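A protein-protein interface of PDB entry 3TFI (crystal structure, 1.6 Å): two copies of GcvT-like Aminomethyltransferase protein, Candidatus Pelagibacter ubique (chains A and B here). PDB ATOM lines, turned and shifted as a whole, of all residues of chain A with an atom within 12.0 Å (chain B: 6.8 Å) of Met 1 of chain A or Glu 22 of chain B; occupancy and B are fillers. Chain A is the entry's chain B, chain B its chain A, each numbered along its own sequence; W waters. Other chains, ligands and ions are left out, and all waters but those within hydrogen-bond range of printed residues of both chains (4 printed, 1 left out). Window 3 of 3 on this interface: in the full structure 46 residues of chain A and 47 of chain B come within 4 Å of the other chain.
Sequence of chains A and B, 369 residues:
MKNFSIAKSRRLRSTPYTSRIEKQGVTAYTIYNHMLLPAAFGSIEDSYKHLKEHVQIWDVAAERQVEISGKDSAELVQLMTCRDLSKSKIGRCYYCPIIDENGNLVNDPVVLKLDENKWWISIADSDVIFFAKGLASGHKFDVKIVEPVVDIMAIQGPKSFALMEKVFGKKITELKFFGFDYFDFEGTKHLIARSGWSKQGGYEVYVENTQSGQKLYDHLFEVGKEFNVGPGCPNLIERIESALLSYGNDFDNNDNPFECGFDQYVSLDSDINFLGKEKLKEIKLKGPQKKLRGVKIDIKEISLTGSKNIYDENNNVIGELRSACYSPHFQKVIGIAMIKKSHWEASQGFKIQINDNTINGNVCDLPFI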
ATOM      1  N   MET A   1      -3.350  25.948   1.236  1.00  0.00           N
ATOM      2  CA  MET A   1      -4.650  25.505   0.648  1.00  0.00           C
ATOM      3  C   MET A   1      -5.747  26.609   0.647  1.00  0.00           C
ATOM      4  O   MET A   1      -6.538  26.799   1.595  1.00  0.00           O
ATOM      5  CB  MET A   1      -5.091  24.124   1.237  1.00  0.00           C
ATOM      6  CG  MET A   1      -6.623  23.749   1.232  1.00  0.00           C
ATOM      7  SD  MET A   1      -7.538  23.304  -0.299  1.00  0.00           S
ATOM      8  CE  MET A   1      -8.991  24.314   0.068  1.00  0.00           C
ATOM      9  N   LYS A   2      -5.714  27.396  -0.442  1.00  0.00           N
ATOM     10  CA  LYS A   2      -6.947  27.924  -1.090  1.00  0.00           C
ATOM     11  C   LYS A   2      -6.786  27.879  -2.637  1.00  0.00           C
ATOM     12  O   LYS A   2      -7.466  27.068  -3.237  1.00  0.00           O
ATOM     13  CB  LYS A   2      -7.470  29.261  -0.697  1.00  0.00           C
ATOM     14  CG  LYS A   2      -8.965  29.355  -0.989  1.00  0.00           C
ATOM     15  CD  LYS A   2      -9.264  30.042  -2.308  1.00  0.00           C
ATOM     16  CE  LYS A   2      -9.914  31.386  -2.167  1.00  0.00           C
ATOM     17  NZ  LYS A   2     -10.119  32.002  -3.542  1.00  0.00           N
ATOM     18  N   ASN A   3      -5.997  28.788  -3.242  1.00  0.00           N
ATOM     19  CA  ASN A   3      -5.526  28.607  -4.606  1.00  0.00           C
ATOM     20  C   ASN A   3      -4.153  27.949  -4.590  1.00  0.00           C
ATOM     21  O   ASN A   3      -3.417  28.016  -3.614  1.00  0.00           O
ATOM     22  CB  ASN A   3      -5.450  29.924  -5.421  1.00  0.00           C
ATOM     23  CG  ASN A   3      -6.820  30.363  -5.915  1.00  0.00           C
ATOM     24  OD1 ASN A   3      -7.636  29.543  -6.330  1.00  0.00           O
ATOM     25  ND2 ASN A   3      -7.114  31.612  -5.753  1.00  0.00           N
ATOM     26  N   PHE A   4      -3.840  27.286  -5.692  1.00  0.00           N
ATOM     27  CA  PHE A   4      -2.563  26.619  -5.957  1.00  0.00           C
ATOM     28  C   PHE A   4      -2.015  27.040  -7.273  1.00  0.00           C
ATOM     29  O   PHE A   4      -2.772  27.239  -8.233  1.00  0.00           O
ATOM     30  CB  PHE A   4      -2.758  25.091  -5.952  1.00  0.00           C
ATOM     31  CG  PHE A   4      -3.385  24.556  -4.673  1.00  0.00           C
ATOM     32  CD1 PHE A   4      -2.613  24.283  -3.572  1.00  0.00           C
ATOM     33  CD2 PHE A   4      -4.757  24.451  -4.556  1.00  0.00           C
ATOM     34  CE1 PHE A   4      -3.178  23.888  -2.416  1.00  0.00           C
ATOM     35  CE2 PHE A   4      -5.328  24.003  -3.408  1.00  0.00           C
ATOM     36  CZ  PHE A   4      -4.544  23.763  -2.324  1.00  0.00           C
ATOM     37  N   SER A   5      -0.687  27.150  -7.354  1.00  0.00           N
ATOM     38  CA  SER A   5      -0.019  27.575  -8.588  1.00  0.00           C
ATOM     39  C   SER A   5       0.039  26.455  -9.563  1.00  0.00           C
ATOM     40  O   SER A   5       0.177  25.286  -9.183  1.00  0.00           O
ATOM     41  CB  SER A   5       1.389  28.090  -8.347  1.00  0.00           C
ATOM     42  OG  SER A   5       1.323  29.266  -7.532  1.00  0.00           O
ATOM     43  N   ILE A   6       0.014  26.798 -10.843  1.00  0.00           N
ATOM     44  CA  ILE A   6       0.351  25.835 -11.878  1.00  0.00           C
ATOM     45  C   ILE A   6       1.867  25.802 -12.045  1.00  0.00           C
ATOM     46  O   ILE A   6       2.523  26.852 -11.993  1.00  0.00           O
ATOM     47  CB  ILE A   6      -0.396  26.186 -13.197  1.00  0.00           C
ATOM     48  CG1 ILE A   6      -0.394  25.032 -14.169  1.00  0.00           C
ATOM     49  CG2 ILE A   6       0.157  27.453 -13.860  1.00  0.00           C
ATOM     50  CD1 ILE A   6      -1.324  25.212 -15.351  1.00  0.00           C
ATOM     51  N   ILE A 302     -20.369  29.076  -4.963  1.00  0.00           N
ATOM     52  CA  ILE A 302     -19.952  27.661  -5.043  1.00  0.00           C
ATOM     53  C   ILE A 302     -18.585  27.592  -5.720  1.00  0.00           C
ATOM     54  O   ILE A 302     -18.264  28.482  -6.536  1.00  0.00           O
ATOM     55  CB  ILE A 302     -20.987  26.818  -5.808  1.00  0.00           C
ATOM     56  CG1 ILE A 302     -20.748  25.334  -5.617  1.00  0.00           C
ATOM     57  CG2 ILE A 302     -20.992  27.183  -7.271  1.00  0.00           C
ATOM     58  CD1 ILE A 302     -21.918  24.459  -5.965  1.00  0.00           C
ATOM     59  N   SER A 303     -17.790  26.575  -5.366  1.00  0.00           N
ATOM     60  CA  SER A 303     -16.492  26.343  -6.028  1.00  0.00           C
ATOM     61  C   SER A 303     -16.431  24.873  -6.321  1.00  0.00           C
ATOM     62  O   SER A 303     -15.873  24.088  -5.521  1.00  0.00           O
ATOM     63  CB  SER A 303     -15.298  26.729  -5.133  1.00  0.00           C
ATOM     64  OG  SER A 303     -14.052  26.483  -5.792  1.00  0.00           O
ATOM     65  N   LEU A 304     -17.014  24.473  -7.455  1.00  0.00           N
ATOM     66  CA  LEU A 304     -17.159  23.067  -7.768  1.00  0.00           C
ATOM     67  C   LEU A 304     -15.892  22.452  -8.388  1.00  0.00           C
ATOM     68  O   LEU A 304     -15.401  22.926  -9.430  1.00  0.00           O
ATOM     69  CB  LEU A 304     -18.388  22.859  -8.663  1.00  0.00           C
ATOM     70  CG  LEU A 304     -18.823  21.405  -8.791  1.00  0.00           C
ATOM     71  CD1 LEU A 304     -19.574  20.873  -7.497  1.00  0.00           C
ATOM     72  CD2 LEU A 304     -19.709  21.261  -9.994  1.00  0.00           C
ATOM     73  N   THR A 305     -15.363  21.403  -7.767  1.00  0.00           N
ATOM     74  CA  THR A 305     -14.082  20.836  -8.232  1.00  0.00           C
ATOM     75  C   THR A 305     -14.226  19.383  -8.717  1.00  0.00           C
ATOM     76  O   THR A 305     -13.235  18.765  -9.116  1.00  0.00           O
ATOM     77  CB  THR A 305     -13.015  20.883  -7.090  1.00  0.00           C
ATOM     78  OG1 THR A 305     -13.417  20.050  -6.005  1.00  0.00           O
ATOM     79  CG2 THR A 305     -12.750  22.295  -6.602  1.00  0.00           C
ATOM     80  N   GLY A 306     -15.403  18.790  -8.597  1.00  0.00           N
ATOM     81  CA  GLY A 306     -15.636  17.401  -8.979  1.00  0.00           C
ATOM     82  C   GLY A 306     -17.116  17.159  -8.736  1.00  0.00           C
ATOM     83  O   GLY A 306     -17.842  18.088  -8.316  1.00  0.00           O
ATOM     84  N   LYS A 308     -20.559  16.278  -7.301  1.00  0.00           N
ATOM     85  CA  LYS A 308     -21.232  16.307  -6.007  1.00  0.00           C
ATOM     86  C   LYS A 308     -22.541  15.559  -6.121  1.00  0.00           C
ATOM     87  O   LYS A 308     -23.336  15.834  -6.994  1.00  0.00           O
ATOM     88  CB  LYS A 308     -21.462  17.749  -5.570  1.00  0.00           C
ATOM     89  CG  LYS A 308     -21.772  18.062  -4.104  1.00  0.00           C
ATOM     90  CD  LYS A 308     -20.434  18.148  -3.308  1.00  0.00           C
ATOM     91  CE  LYS A 308     -20.434  19.171  -2.175  1.00  0.00           C
ATOM     92  NZ  LYS A 308     -19.962  20.520  -2.621  1.00  0.00           N
ATOM     93  N   ASN A 355     -21.033  22.095   2.950  1.00  0.00           N
ATOM     94  CA  ASN A 355     -20.458  22.346   4.280  1.00  0.00           C
ATOM     95  C   ASN A 355     -21.479  22.140   5.403  1.00  0.00           C
ATOM     96  O   ASN A 355     -22.084  21.075   5.486  1.00  0.00           O
ATOM     97  CB  ASN A 355     -19.834  23.756   4.317  1.00  0.00           C
ATOM     98  CG  ASN A 355     -18.662  23.897   3.387  1.00  0.00           C
ATOM     99  OD1 ASN A 355     -17.671  23.134   3.471  1.00  0.00           O
ATOM    100  ND2 ASN A 355     -18.745  24.890   2.492  1.00  0.00           N
ATOM    101  N   LYS B   8      -9.477  24.709 -10.912  1.00  0.00           N
ATOM    102  CA  LYS B   8     -10.034  23.376 -10.760  1.00  0.00           C
ATOM    103  C   LYS B   8     -11.403  23.228 -11.429  1.00  0.00           C
ATOM    104  O   LYS B   8     -12.124  24.225 -11.589  1.00  0.00           O
ATOM    105  CB  LYS B   8     -10.128  23.018  -9.291  1.00  0.00           C
ATOM    106  CG  LYS B   8      -8.753  22.863  -8.597  1.00  0.00           C
ATOM    107  CD  LYS B   8      -8.918  22.321  -7.323  1.00  0.00           C
ATOM    108  CE  LYS B   8      -7.569  22.058  -6.709  1.00  0.00           C
ATOM    109  NZ  LYS B   8      -8.002  21.594  -5.366  1.00  0.00           N
ATOM    110  N   SER B  14      -9.703  15.509  -9.627  1.00  0.00           N
ATOM    111  CA  SER B  14      -9.069  15.335  -8.327  1.00  0.00           C
ATOM    112  C   SER B  14      -8.858  13.827  -8.108  1.00  0.00           C
ATOM    113  O   SER B  14      -9.253  12.959  -8.914  1.00  0.00           O
ATOM    114  CB  SER B  14      -9.843  16.085  -7.225  1.00  0.00           C
ATOM    115  OG  SER B  14      -9.691  17.530  -7.310  1.00  0.00           O
ATOM    116  N   TYR B  17      -6.483  11.293  -2.922  1.00  0.00           N
ATOM    117  CA  TYR B  17      -5.519  11.839  -1.997  1.00  0.00           C
ATOM    118  C   TYR B  17      -5.544  13.362  -1.975  1.00  0.00           C
ATOM    119  O   TYR B  17      -4.831  13.957  -1.148  1.00  0.00           O
ATOM    120  CB  TYR B  17      -4.114  11.330  -2.290  1.00  0.00           C
ATOM    121  CG  TYR B  17      -4.044   9.825  -2.585  1.00  0.00           C
ATOM    122  CD1 TYR B  17      -4.373   8.879  -1.626  1.00  0.00           C
ATOM    123  CD2 TYR B  17      -3.809   9.350  -3.872  1.00  0.00           C
ATOM    124  CE1 TYR B  17      -4.348   7.532  -1.911  1.00  0.00           C
ATOM    125  CE2 TYR B  17      -3.811   8.007  -4.170  1.00  0.00           C
ATOM    126  CZ  TYR B  17      -4.114   7.081  -3.187  1.00  0.00           C
ATOM    127  OH  TYR B  17      -4.151   5.710  -3.403  1.00  0.00           O
ATOM    128  N   THR B  18      -6.316  14.009  -2.858  1.00  0.00           N
ATOM    129  CA  THR B  18      -6.305  15.496  -2.950  1.00  0.00           C
ATOM    130  C   THR B  18      -6.562  16.203  -1.644  1.00  0.00           C
ATOM    131  O   THR B  18      -5.796  17.102  -1.231  1.00  0.00           O
ATOM    132  CB  THR B  18      -7.362  15.962  -3.960  1.00  0.00           C
ATOM    133  OG1 THR B  18      -7.018  15.425  -5.246  1.00  0.00           O
ATOM    134  CG2 THR B  18      -7.434  17.522  -3.994  1.00  0.00           C
ATOM    135  N   SER B  19      -7.615  15.783  -0.929  1.00  0.00           N
ATOM    136  CA  SER B  19      -7.907  16.462   0.319  1.00  0.00           C
ATOM    137  C   SER B  19      -6.809  16.323   1.337  1.00  0.00           C
ATOM    138  O   SER B  19      -6.553  17.266   2.088  1.00  0.00           O
ATOM    139  CB  SER B  19      -9.288  16.032   0.853  1.00  0.00           C
ATOM    140  OG  SER B  19      -9.350  14.682   1.306  1.00  0.00           O
ATOM    141  N   ARG B  20      -6.139  15.181   1.336  1.00  0.00           N
ATOM    142  CA  ARG B  20      -5.030  14.965   2.238  1.00  0.00           C
ATOM    143  C   ARG B  20      -3.818  15.857   1.873  1.00  0.00           C
ATOM    144  O   ARG B  20      -3.233  16.514   2.743  1.00  0.00           O
ATOM    145  CB  ARG B  20      -4.657  13.490   2.241  1.00  0.00           C
ATOM    146  CG  ARG B  20      -5.648  12.636   3.052  1.00  0.00           C
ATOM    147  CD  ARG B  20      -5.555  11.165   2.638  1.00  0.00           C
ATOM    148  NE  ARG B  20      -6.314  10.334   3.555  1.00  0.00           N
ATOM    149  CZ  ARG B  20      -7.633  10.174   3.563  1.00  0.00           C
ATOM    150  NH1 ARG B  20      -8.423  10.654   2.630  1.00  0.00           N
ATOM    151  NH2 ARG B  20      -8.189   9.476   4.557  1.00  0.00           N
ATOM    152  N   ILE B  21      -3.389  15.804   0.622  1.00  0.00           N
ATOM    153  CA  ILE B  21      -2.202  16.545   0.250  1.00  0.00           C
ATOM    154  C   ILE B  21      -2.377  18.058   0.401  1.00  0.00           C
ATOM    155  O   ILE B  21      -1.410  18.797   0.640  1.00  0.00           O
ATOM    156  CB  ILE B  21      -1.629  16.153  -1.126  1.00  0.00           C
ATOM    157  CG1 ILE B  21      -2.512  16.553  -2.323  1.00  0.00           C
ATOM    158  CG2 ILE B  21      -1.287  14.628  -1.132  1.00  0.00           C
ATOM    159  CD1 ILE B  21      -1.826  16.301  -3.674  1.00  0.00           C
ATOM    160  N   GLU B  22      -3.597  18.535   0.243  1.00  0.00           N
ATOM    161  CA  GLU B  22      -3.873  19.964   0.430  1.00  0.00           C
ATOM    162  C   GLU B  22      -3.874  20.336   1.873  1.00  0.00           C
ATOM    163  O   GLU B  22      -3.896  21.539   2.167  1.00  0.00           O
ATOM    164  CB  GLU B  22      -5.176  20.357  -0.310  1.00  0.00           C
ATOM    165  CG  GLU B  22      -5.034  20.269  -1.815  1.00  0.00           C
ATOM    166  CD  GLU B  22      -6.180  20.715  -2.658  1.00  0.00           C
ATOM    167  OE1 GLU B  22      -7.236  21.155  -2.138  1.00  0.00           O
ATOM    168  OE2 GLU B  22      -5.976  20.628  -3.929  1.00  0.00           O
ATOM    169  N   LYS B  23      -3.954  19.410   2.812  1.00  0.00           N
ATOM    170  CA  LYS B  23      -3.642  19.722   4.208  1.00  0.00           C
ATOM    171  C   LYS B  23      -2.174  19.457   4.595  1.00  0.00           C
ATOM    172  O   LYS B  23      -1.734  19.808   5.713  1.00  0.00           O
ATOM    173  CB  LYS B  23      -4.587  18.833   5.066  1.00  0.00           C
ATOM    174  CG  LYS B  23      -6.042  19.315   5.048  1.00  0.00           C
ATOM    175  CD  LYS B  23      -7.084  18.371   5.689  1.00  0.00           C
ATOM    176  CE  LYS B  23      -6.964  16.902   5.151  1.00  0.00           C
ATOM    177  NZ  LYS B  23      -8.234  16.261   4.699  1.00  0.00           N
ATOM    178  N   GLN B  24      -1.385  18.874   3.701  1.00  0.00           N
ATOM    179  CA  GLN B  24       0.001  18.524   3.946  1.00  0.00           C
ATOM    180  C   GLN B  24       1.002  19.425   3.211  1.00  0.00           C
ATOM    181  O   GLN B  24       2.200  19.093   3.079  1.00  0.00           O
ATOM    182  CB  GLN B  24       0.248  17.071   3.608  1.00  0.00           C
ATOM    183  CG  GLN B  24      -0.465  16.107   4.505  1.00  0.00           C
ATOM    184  CD  GLN B  24      -0.328  14.708   4.044  1.00  0.00           C
ATOM    185  OE1 GLN B  24      -0.806  14.395   2.982  1.00  0.00           O
ATOM    186  NE2 GLN B  24       0.273  13.824   4.872  1.00  0.00           N
ATOM    187  N   GLY B  25       0.507  20.511   2.625  1.00  0.00           N
ATOM    188  CA  GLY B  25       1.421  21.478   2.087  1.00  0.00           C
ATOM    189  C   GLY B  25       1.678  21.544   0.624  1.00  0.00           C
ATOM    190  O   GLY B  25       2.664  22.111   0.227  1.00  0.00           O
ATOM    191  N   VAL B  26       0.844  20.919  -0.204  1.00  0.00           N
ATOM    192  CA  VAL B  26       1.086  21.034  -1.638  1.00  0.00           C
ATOM    193  C   VAL B  26       1.041  22.511  -2.024  1.00  0.00           C
ATOM    194  O   VAL B  26       0.188  23.281  -1.550  1.00  0.00           O
ATOM    195  CB  VAL B  26       0.145  20.150  -2.493  1.00  0.00           C
ATOM    196  CG1 VAL B  26      -1.331  20.658  -2.423  1.00  0.00           C
ATOM    197  CG2 VAL B  26       0.669  20.016  -3.936  1.00  0.00           C
ATOM    198  N   TYR B  29       0.666  22.481  -8.636  1.00  0.00           N
ATOM    199  CA  TYR B  29       0.132  21.324  -9.409  1.00  0.00           C
ATOM    200  C   TYR B  29       0.567  21.389 -10.859  1.00  0.00           C
ATOM    201  O   TYR B  29       0.680  22.482 -11.462  1.00  0.00           O
ATOM    202  CB  TYR B  29      -1.382  21.280  -9.375  1.00  0.00           C
ATOM    203  CG  TYR B  29      -1.994  20.767  -8.099  1.00  0.00           C
ATOM    204  CD1 TYR B  29      -1.915  19.419  -7.777  1.00  0.00           C
ATOM    205  CD2 TYR B  29      -2.733  21.595  -7.262  1.00  0.00           C
ATOM    206  CE1 TYR B  29      -2.571  18.919  -6.675  1.00  0.00           C
ATOM    207  CE2 TYR B  29      -3.386  21.116  -6.167  1.00  0.00           C
ATOM    208  CZ  TYR B  29      -3.320  19.757  -5.863  1.00  0.00           C
ATOM    209  OH  TYR B  29      -3.980  19.188  -4.784  1.00  0.00           O
ATOM    210  N   LEU B  36      -5.047  16.062 -11.601  1.00  0.00           N
ATOM    211  CA  LEU B  36      -4.126  16.820 -10.772  1.00  0.00           C
ATOM    212  C   LEU B  36      -2.985  15.907 -10.307  1.00  0.00           C
ATOM    213  O   LEU B  36      -3.238  14.825  -9.781  1.00  0.00           O
ATOM    214  CB  LEU B  36      -4.869  17.349  -9.540  1.00  0.00           C
ATOM    215  CG  LEU B  36      -5.885  18.456  -9.829  1.00  0.00           C
ATOM    216  CD1 LEU B  36      -6.804  18.679  -8.576  1.00  0.00           C
ATOM    217  CD2 LEU B  36      -5.112  19.739 -10.208  1.00  0.00           C
ATOM    218  N   PHE B  41       5.875  20.660  -3.086  1.00  0.00           N
ATOM    219  CA  PHE B  41       5.555  20.870  -1.677  1.00  0.00           C
ATOM    220  C   PHE B  41       6.642  21.824  -1.155  1.00  0.00           C
ATOM    221  O   PHE B  41       7.542  21.447  -0.385  1.00  0.00           O
ATOM    222  CB  PHE B  41       5.585  19.552  -0.856  1.00  0.00           C
ATOM    223  CG  PHE B  41       4.464  18.601  -1.202  1.00  0.00           C
ATOM    224  CD1 PHE B  41       4.520  17.814  -2.333  1.00  0.00           C
ATOM    225  CD2 PHE B  41       3.315  18.523  -0.393  1.00  0.00           C
ATOM    226  CE1 PHE B  41       3.473  16.943  -2.679  1.00  0.00           C
ATOM    227  CE2 PHE B  41       2.316  17.662  -0.679  1.00  0.00           C
ATOM    228  CZ  PHE B  41       2.361  16.875  -1.845  1.00  0.00           C
HETATM  229  O   HOH W   1     -10.542  19.246  -9.503  1.00  0.00           O
HETATM  230  O   HOH W   2     -12.431  16.290  -9.658  1.00  0.00           O
HETATM  231  O   HOH W   3      -1.339  23.377   0.720  1.00  0.00           O
HETATM  232  O   HOH W   4      -9.084  19.929  -0.642  1.00  0.00           O
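N of Tyr 29 of chain B sits at hydrogen-bond distance from O of Ser 5 of chain A.
The side-chain sulfur (SD) of Met 1 of chain A sits close to the side-chain carboxylate (OE1) of Glu 22 of chain B, 2.8 Å away.
The side-chain amino group of Lys 8 of chain B lies within salt-bridge range of the side-chain carboxylate of Glu 22 of chain B (2.7 Å).
O of Ile 21 of chain B is in hydrogen-bond range of N of Val 26 of chain B.
OH of Tyr 29 of chain B is in hydrogen-bond range of OE2 of Glu 22 of chain B.
Phe 4 of chain A touches Glu 22 of chain B.
Val 26 of chain B touches Phe 4 of chain A.
CD2 of Tyr 29 of chain B touches CB of Phe 4 of chain A, at 3.7 Å.
Ile 6 of chain A touches Tyr 29 of chain B.
Thr 305 of chain A touches Lys 8 of chain B (CG2 to CB, 3.8 Å).
Of the printed residues of chain B, Met 1 of chain A touches Glu 22 (2.8 Å).
Printed residues of chain A within 4 Å of Glu 22 of chain B: Met 1 (2.8 Å) and Phe 4 (3.5 Å).
No residue of chain A comes within 4 Å of Thr 18 of chain B.
No residue of chain A comes within 4 Å of Ser 19 of chain B.
No residue of chain A comes within 4 Å of Gln 24 of chain B.
Printed residues of chain A within 4 Å of Val 26 of chain B: Phe 4.
Of the printed residues of chain A, Tyr 29 of chain B touches Phe 4 (3.7 Å), Ser 5 (2.9 Å) and Ile 6 (3.4 Å).
Of the printed residues of chain A, Lys 8 of chain B touches Thr 305.
Printed residues of chain B within 4 Å of Ser 5 of chain A: Tyr 29 (2.9 Å).
Leu 36 of chain B touches none of the printed residues of chain A.
The nearest printed residue of chain B that does not touch Met 1 of chain A is Lys 23 of chain B (5.1 Å).
Hydrophobic or aromatic side chains of chain A that line the printed part of chain B: Met 1, Phe 4 and Ile 6.
Along chain A the printed residues that touch a printed residue of chain B span positions 1 to 305.
Of the 15 printed residues of chain B, 4 touch a printed residue of chain A.
Printed residues of chain B that touch a printed residue of chain A: Lys 8, Glu 22, Val 26 and Tyr 29.
No position is printed for both chains.
Water W2 lies within hydrogen-bond range of O of Thr 305 of chain A and N of Ser 14 of chain B.
Water W4 lies within hydrogen-bond range of OE1 of Glu 22 of chain B (2.7 Å) and SD of Met 1 of chain A (3.7 Å).
Water W3 lies within hydrogen-bond range of the backbone carbonyl oxygen (O) of Val 26 of chain B (2.7 Å), the backbone NH (N) of Met 1 of chain A (3.3 Å) and the backbone carbonyl oxygen (O) of Glu 22 of chain B (3.5 Å).
Water W1 lies within hydrogen-bond range of O of Thr 305 of chain A (2.8 Å) and OG of Ser 14 of chain B (2.9 Å).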
